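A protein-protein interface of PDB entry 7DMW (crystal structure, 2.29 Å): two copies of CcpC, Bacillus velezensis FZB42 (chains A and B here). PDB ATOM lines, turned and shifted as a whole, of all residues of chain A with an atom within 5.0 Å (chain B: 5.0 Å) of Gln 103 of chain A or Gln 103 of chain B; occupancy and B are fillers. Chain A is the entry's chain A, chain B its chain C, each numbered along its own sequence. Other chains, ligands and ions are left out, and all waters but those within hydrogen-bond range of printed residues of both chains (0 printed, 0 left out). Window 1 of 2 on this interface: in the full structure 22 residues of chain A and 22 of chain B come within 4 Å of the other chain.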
ATOM      1  N   SER A  99      19.013 -24.676   8.206  1.00  0.00           N
ATOM      2  CA  SER A  99      19.532 -23.591   9.050  1.00  0.00           C
ATOM      3  C   SER A  99      20.207 -24.111  10.303  1.00  0.00           C
ATOM      4  O   SER A  99      21.358 -23.767  10.572  1.00  0.00           O
ATOM      5  CB  SER A  99      18.417 -22.625   9.439  1.00  0.00           C
ATOM      6  OG  SER A  99      17.978 -21.914   8.302  1.00  0.00           O
ATOM      7  N   ILE A 100      19.511 -24.930  11.096  1.00  0.00           N
ATOM      8  CA  ILE A 100      20.118 -25.378  12.347  1.00  0.00           C
ATOM      9  C   ILE A 100      21.372 -26.194  12.078  1.00  0.00           C
ATOM     10  O   ILE A 100      22.313 -26.184  12.880  1.00  0.00           O
ATOM     11  CB  ILE A 100      19.112 -26.164  13.208  1.00  0.00           C
ATOM     12  CG1 ILE A 100      18.564 -27.362  12.433  1.00  0.00           C
ATOM     13  CG2 ILE A 100      18.003 -25.263  13.603  1.00  0.00           C
ATOM     14  CD1 ILE A 100      17.962 -28.442  13.297  1.00  0.00           C
ATOM     15  N   ILE A 101      21.424 -26.892  10.945  1.00  0.00           N
ATOM     16  CA  ILE A 101      22.643 -27.598  10.584  1.00  0.00           C
ATOM     17  C   ILE A 101      23.742 -26.597  10.269  1.00  0.00           C
ATOM     18  O   ILE A 101      24.883 -26.734  10.733  1.00  0.00           O
ATOM     19  CB  ILE A 101      22.399 -28.555   9.401  1.00  0.00           C
ATOM     20  CG1 ILE A 101      21.399 -29.642   9.792  1.00  0.00           C
ATOM     21  CG2 ILE A 101      23.724 -29.153   8.962  1.00  0.00           C
ATOM     22  CD1 ILE A 101      21.920 -30.532  10.913  1.00  0.00           C
ATOM     23  N   GLY A 102      23.416 -25.580   9.468  1.00  0.00           N
ATOM     24  CA  GLY A 102      24.407 -24.571   9.116  1.00  0.00           C
ATOM     25  C   GLY A 102      25.009 -23.878  10.327  1.00  0.00           C
ATOM     26  O   GLY A 102      26.168 -23.465  10.307  1.00  0.00           O
ATOM     27  N   GLN A 103      24.249 -23.777  11.401  1.00  0.00           N
ATOM     28  CA  GLN A 103      24.663 -23.065  12.593  1.00  0.00           C
ATOM     29  C   GLN A 103      25.442 -23.940  13.548  1.00  0.00           C
ATOM     30  O   GLN A 103      26.424 -23.478  14.141  1.00  0.00           O
ATOM     31  CB  GLN A 103      23.436 -22.527  13.312  1.00  0.00           C
ATOM     32  CG  GLN A 103      22.835 -21.335  12.619  1.00  0.00           C
ATOM     33  CD  GLN A 103      22.356 -20.332  13.630  1.00  0.00           C
ATOM     34  OE1 GLN A 103      22.940 -20.220  14.721  1.00  0.00           O
ATOM     35  NE2 GLN A 103      21.307 -19.590  13.291  1.00  0.00           N
ATOM     36  N   HIS A 104      25.000 -25.191  13.709  1.00  0.00           N
ATOM     37  CA  HIS A 104      25.363 -25.998  14.854  1.00  0.00           C
ATOM     38  C   HIS A 104      26.249 -27.196  14.525  1.00  0.00           C
ATOM     39  O   HIS A 104      26.914 -27.715  15.422  1.00  0.00           O
ATOM     40  CB  HIS A 104      24.093 -26.503  15.549  1.00  0.00           C
ATOM     41  CG  HIS A 104      23.354 -25.441  16.294  1.00  0.00           C
ATOM     42  ND1 HIS A 104      23.789 -24.946  17.504  1.00  0.00           N
ATOM     43  CD2 HIS A 104      22.209 -24.778  16.006  1.00  0.00           C
ATOM     44  CE1 HIS A 104      22.944 -24.022  17.928  1.00  0.00           C
ATOM     45  NE2 HIS A 104      21.976 -23.900  17.036  1.00  0.00           N
ATOM     46  N   TRP A 105      26.281 -27.637  13.289  1.00  0.00           N
ATOM     47  CA  TRP A 105      27.003 -28.836  12.908  1.00  0.00           C
ATOM     48  C   TRP A 105      28.001 -28.582  11.803  1.00  0.00           C
ATOM     49  O   TRP A 105      29.105 -29.133  11.846  1.00  0.00           O
ATOM     50  CB  TRP A 105      26.004 -29.905  12.460  1.00  0.00           C
ATOM     51  CG  TRP A 105      26.632 -31.181  12.144  1.00  0.00           C
ATOM     52  CD1 TRP A 105      27.006 -32.144  13.028  1.00  0.00           C
ATOM     53  CD2 TRP A 105      26.968 -31.674  10.840  1.00  0.00           C
ATOM     54  NE1 TRP A 105      27.560 -33.205  12.363  1.00  0.00           N
ATOM     55  CE2 TRP A 105      27.539 -32.949  11.015  1.00  0.00           C
ATOM     56  CE3 TRP A 105      26.842 -31.162   9.544  1.00  0.00           C
ATOM     57  CZ2 TRP A 105      27.986 -33.721   9.945  1.00  0.00           C
ATOM     58  CZ3 TRP A 105      27.282 -31.927   8.485  1.00  0.00           C
ATOM     59  CH2 TRP A 105      27.850 -33.191   8.691  1.00  0.00           C
ATOM     60  N   PRO A 107      29.836 -25.713  10.954  1.00  0.00           N
ATOM     61  CA  PRO A 107      31.122 -25.052  11.264  1.00  0.00           C
ATOM     62  C   PRO A 107      32.288 -26.006  11.492  1.00  0.00           C
ATOM     63  O   PRO A 107      33.355 -25.827  10.881  1.00  0.00           O
ATOM     64  CB  PRO A 107      30.793 -24.248  12.523  1.00  0.00           C
ATOM     65  CG  PRO A 107      29.386 -23.809  12.298  1.00  0.00           C
ATOM     66  CD  PRO A 107      28.712 -25.033  11.641  1.00  0.00           C
ATOM     67  N   GLU A 219      16.356 -21.309  15.922  1.00  0.00           N
ATOM     68  CA  GLU A 219      17.320 -20.658  16.810  1.00  0.00           C
ATOM     69  C   GLU A 219      16.684 -19.519  17.608  1.00  0.00           C
ATOM     70  O   GLU A 219      17.070 -19.269  18.757  1.00  0.00           O
ATOM     71  CB  GLU A 219      18.511 -20.147  15.995  1.00  0.00           C
ATOM     72  CG  GLU A 219      19.590 -19.456  16.818  1.00  0.00           C
ATOM     73  CD  GLU A 219      20.273 -20.396  17.809  1.00  0.00           C
ATOM     74  OE1 GLU A 219      20.566 -21.559  17.452  1.00  0.00           O
ATOM     75  OE2 GLU A 219      20.519 -19.955  18.956  1.00  0.00           O
ATOM     76  N   THR A 220      15.712 -18.820  17.025  1.00  0.00           N
ATOM     77  CA  THR A 220      15.001 -17.810  17.785  1.00  0.00           C
ATOM     78  C   THR A 220      14.191 -18.449  18.907  1.00  0.00           C
ATOM     79  O   THR A 220      14.074 -17.880  19.998  1.00  0.00           O
ATOM     80  CB  THR A 220      14.134 -16.979  16.834  1.00  0.00           C
ATOM     81  OG1 THR A 220      14.999 -16.216  15.972  1.00  0.00           O
ATOM     82  CG2 THR A 220      13.242 -16.011  17.605  1.00  0.00           C
ATOM     83  N   GLN A 223      16.760 -19.066  21.709  1.00  0.00           N
ATOM     84  CA  GLN A 223      17.051 -17.790  22.367  1.00  0.00           C
ATOM     85  C   GLN A 223      15.886 -17.345  23.242  1.00  0.00           C
ATOM     86  O   GLN A 223      16.046 -17.131  24.449  1.00  0.00           O
ATOM     87  CB  GLN A 223      17.366 -16.714  21.329  1.00  0.00           C
ATOM     88  CG  GLN A 223      18.768 -16.739  20.824  1.00  0.00           C
ATOM     89  CD  GLN A 223      19.713 -17.343  21.831  1.00  0.00           C
ATOM     90  OE1 GLN A 223      19.903 -16.803  22.925  1.00  0.00           O
ATOM     91  NE2 GLN A 223      20.314 -18.488  21.471  1.00  0.00           N
ATOM     92  N   SER B  99      16.981 -10.683  10.662  1.00  0.00           N
ATOM     93  CA  SER B  99      17.388 -11.907  11.372  1.00  0.00           C
ATOM     94  C   SER B  99      18.196 -11.598  12.627  1.00  0.00           C
ATOM     95  O   SER B  99      17.814 -12.006  13.726  1.00  0.00           O
ATOM     96  CB  SER B  99      18.184 -12.863  10.470  1.00  0.00           C
ATOM     97  OG  SER B  99      17.625 -13.029   9.175  1.00  0.00           O
ATOM     98  N   ILE B 100      19.303 -10.854  12.495  1.00  0.00           N
ATOM     99  CA  ILE B 100      20.154 -10.626  13.671  1.00  0.00           C
ATOM    100  C   ILE B 100      19.401  -9.907  14.784  1.00  0.00           C
ATOM    101  O   ILE B 100      19.646 -10.158  15.971  1.00  0.00           O
ATOM    102  CB  ILE B 100      21.449  -9.866  13.301  1.00  0.00           C
ATOM    103  CG1 ILE B 100      21.129  -8.586  12.533  1.00  0.00           C
ATOM    104  CG2 ILE B 100      22.374 -10.750  12.504  1.00  0.00           C
ATOM    105  CD1 ILE B 100      22.320  -7.693  12.264  1.00  0.00           C
ATOM    106  N   ILE B 101      18.480  -9.005  14.440  1.00  0.00           N
ATOM    107  CA  ILE B 101      17.678  -8.371  15.480  1.00  0.00           C
ATOM    108  C   ILE B 101      16.794  -9.406  16.174  1.00  0.00           C
ATOM    109  O   ILE B 101      16.688  -9.433  17.406  1.00  0.00           O
ATOM    110  CB  ILE B 101      16.839  -7.221  14.898  1.00  0.00           C
ATOM    111  CG1 ILE B 101      17.723  -6.213  14.150  1.00  0.00           C
ATOM    112  CG2 ILE B 101      16.076  -6.576  16.001  1.00  0.00           C
ATOM    113  CD1 ILE B 101      18.965  -5.732  14.941  1.00  0.00           C
ATOM    114  N   GLY B 102      16.138 -10.266  15.392  1.00  0.00           N
ATOM    115  CA  GLY B 102      15.251 -11.253  15.986  1.00  0.00           C
ATOM    116  C   GLY B 102      15.953 -12.132  17.000  1.00  0.00           C
ATOM    117  O   GLY B 102      15.357 -12.543  17.998  1.00  0.00           O
ATOM    118  N   GLN B 103      17.238 -12.387  16.787  1.00  0.00           N
ATOM    119  CA  GLN B 103      17.952 -13.346  17.608  1.00  0.00           C
ATOM    120  C   GLN B 103      18.591 -12.711  18.821  1.00  0.00           C
ATOM    121  O   GLN B 103      18.597 -13.309  19.903  1.00  0.00           O
ATOM    122  CB  GLN B 103      19.032 -14.027  16.776  1.00  0.00           C
ATOM    123  CG  GLN B 103      18.594 -15.311  16.113  1.00  0.00           C
ATOM    124  CD  GLN B 103      19.781 -16.204  15.880  1.00  0.00           C
ATOM    125  OE1 GLN B 103      20.668 -16.289  16.737  1.00  0.00           O
ATOM    126  NE2 GLN B 103      19.835 -16.851  14.710  1.00  0.00           N
ATOM    127  N   HIS B 104      19.150 -11.517  18.647  1.00  0.00           N
ATOM    128  CA  HIS B 104      19.984 -10.908  19.663  1.00  0.00           C
ATOM    129  C   HIS B 104      19.272  -9.829  20.468  1.00  0.00           C
ATOM    130  O   HIS B 104      19.413  -9.799  21.692  1.00  0.00           O
ATOM    131  CB  HIS B 104      21.245 -10.340  19.004  1.00  0.00           C
ATOM    132  CG  HIS B 104      22.138 -11.394  18.411  1.00  0.00           C
ATOM    133  ND1 HIS B 104      23.202 -11.942  19.096  1.00  0.00           N
ATOM    134  CD2 HIS B 104      22.111 -12.012  17.205  1.00  0.00           C
ATOM    135  CE1 HIS B 104      23.797 -12.844  18.334  1.00  0.00           C
ATOM    136  NE2 HIS B 104      23.154 -12.906  17.182  1.00  0.00           N
ATOM    137  N   TRP B 105      18.483  -8.966  19.821  1.00  0.00           N
ATOM    138  CA  TRP B 105      17.843  -7.814  20.460  1.00  0.00           C
ATOM    139  C   TRP B 105      16.388  -8.069  20.811  1.00  0.00           C
ATOM    140  O   TRP B 105      15.956  -7.723  21.912  1.00  0.00           O
ATOM    141  CB  TRP B 105      17.939  -6.590  19.541  1.00  0.00           C
ATOM    142  CG  TRP B 105      17.380  -5.258  20.061  1.00  0.00           C
ATOM    143  CD1 TRP B 105      18.026  -4.345  20.857  1.00  0.00           C
ATOM    144  CD2 TRP B 105      16.107  -4.672  19.744  1.00  0.00           C
ATOM    145  NE1 TRP B 105      17.223  -3.240  21.075  1.00  0.00           N
ATOM    146  CE2 TRP B 105      16.040  -3.417  20.407  1.00  0.00           C
ATOM    147  CE3 TRP B 105      15.008  -5.089  18.979  1.00  0.00           C
ATOM    148  CZ2 TRP B 105      14.922  -2.584  20.324  1.00  0.00           C
ATOM    149  CZ3 TRP B 105      13.895  -4.252  18.893  1.00  0.00           C
ATOM    150  CH2 TRP B 105      13.861  -3.014  19.568  1.00  0.00           C
ATOM    151  N   PRO B 107      14.634 -10.841  21.707  1.00  0.00           N
ATOM    152  CA  PRO B 107      14.173 -11.689  22.821  1.00  0.00           C
ATOM    153  C   PRO B 107      14.000 -10.937  24.131  1.00  0.00           C
ATOM    154  O   PRO B 107      13.071 -11.250  24.893  1.00  0.00           O
ATOM    155  CB  PRO B 107      15.261 -12.766  22.910  1.00  0.00           C
ATOM    156  CG  PRO B 107      15.743 -12.882  21.544  1.00  0.00           C
ATOM    157  CD  PRO B 107      15.758 -11.483  20.999  1.00  0.00           C
ATOM    158  N   GLU B 219      24.634 -14.734  11.413  1.00  0.00           N
ATOM    159  CA  GLU B 219      24.935 -15.616  12.542  1.00  0.00           C
ATOM    160  C   GLU B 219      25.824 -16.798  12.126  1.00  0.00           C
ATOM    161  O   GLU B 219      26.632 -17.285  12.928  1.00  0.00           O
ATOM    162  CB  GLU B 219      23.628 -16.104  13.172  1.00  0.00           C
ATOM    163  CG  GLU B 219      23.778 -17.117  14.305  1.00  0.00           C
ATOM    164  CD  GLU B 219      24.346 -16.501  15.571  1.00  0.00           C
ATOM    165  OE1 GLU B 219      24.255 -15.255  15.723  1.00  0.00           O
ATOM    166  OE2 GLU B 219      24.886 -17.271  16.408  1.00  0.00           O
ATOM    167  N   THR B 220      25.719 -17.250  10.875  1.00  0.00           N
ATOM    168  CA  THR B 220      26.604 -18.314  10.415  1.00  0.00           C
ATOM    169  C   THR B 220      28.040 -17.826  10.321  1.00  0.00           C
ATOM    170  O   THR B 220      28.973 -18.570  10.656  1.00  0.00           O
ATOM    171  CB  THR B 220      26.131 -18.861   9.071  1.00  0.00           C
ATOM    172  OG1 THR B 220      24.852 -19.469   9.248  1.00  0.00           O
ATOM    173  CG2 THR B 220      27.080 -19.945   8.580  1.00  0.00           C
ATOM    174  N   GLN B 223      29.434 -17.838  13.957  1.00  0.00           N
ATOM    175  CA  GLN B 223      29.801 -19.185  14.400  1.00  0.00           C
ATOM    176  C   GLN B 223      31.098 -19.645  13.747  1.00  0.00           C
ATOM    177  O   GLN B 223      32.014 -20.117  14.426  1.00  0.00           O
ATOM    178  CB  GLN B 223      28.674 -20.179  14.110  1.00  0.00           C
ATOM    179  CG  GLN B 223      27.450 -20.023  15.000  1.00  0.00           C
ATOM    180  CD  GLN B 223      27.805 -19.919  16.473  1.00  0.00           C
ATOM    181  OE1 GLN B 223      28.554 -20.735  16.990  1.00  0.00           O
ATOM    182  NE2 GLN B 223      27.282 -18.891  17.150  1.00  0.00           N
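NE2 of Gln 103 of chain A lies close to NE2 of Gln 103 of chain B (3.4 Å).
The side-chain carboxylate of Glu 219 of chain B sits at hydrogen-bond distance from the side-chain amide nitrogen of Gln 223 of chain B (3.0 Å). OE2 of Glu 219 of chain A sits at hydrogen-bond distance from NE2 of Gln 223 of chain A. NE2 of His 104 of chain B sits at hydrogen-bond distance from OE1 of Glu 219 of chain B (3.0 Å). NE2 of His 104 of chain A sits at hydrogen-bond distance from OE1 of Glu 219 of chain A, at 2.8 Å.
Gln 103 of chain A touches Glu 219 of chain B. Gln 103 of chain A touches Gln 223 of chain B (O to CG, 3.7 Å). OE1 of Gln 103 of chain B touches CG of Glu 219 of chain A, at 3.3 Å. Gln 103 of chain B touches Thr 220 of chain A (CG to OG1, 3.7 Å). O of Gln 103 of chain B touches CG of Gln 223 of chain A, 3.6 Å away.
Gln 103 of chain A touches three residues of chain B. Of chain A, only Gln 103, Glu 219, Thr 220 and Gln 223 come within 4 Å of Gln 103 of chain B. Of the printed residues of chain A, Glu 219 of chain B touches Gln 103. Printed residues of chain B within 4 Å of Glu 219 of chain A: Gln 103. Of the printed residues of chain A, Gln 223 of chain B touches Gln 103. Ile 101 of chain A touches none of the printed residues of chain B. Gly 102 of chain B touches none of the printed residues of chain A. The nearest printed residue of chain A that does not touch Gln 223 of chain B is Pro 107 of chain A (4.1 Å).
Printed residues of chain A that touch a printed residue of chain B: Gln 103, Glu 219, Thr 220 and Gln 223. Among the printed residues, no Asp or Glu carboxylate lies within 4 Å of a Lys or Arg side-chain nitrogen of the other chain.
Gln 103 of chain A touches its own counterpart, Gln 103 of chain B. Gln 103 of chain A touches Glu 219 of chain B, and with the chains exchanged Glu 219 of chain A touches Gln 103 of chain B. Gln 103 of chain A touches Gln 223 of chain B, and with the chains exchanged Gln 223 of chain A touches Gln 103 of chain B. Thr 220 of chain A touches Gln 103 of chain B, but with the chains exchanged Gln 103 of chain A does not touch Thr 220 of chain B (4.3 Å). Positions printed for both chains: 99, 100, 101, 102, 103, 104, 105, 107, 219, 220 and 223. Of the 6 pairs that touch across the chains among the printed residues, 5 have their exchanged pair printed and touching as well.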
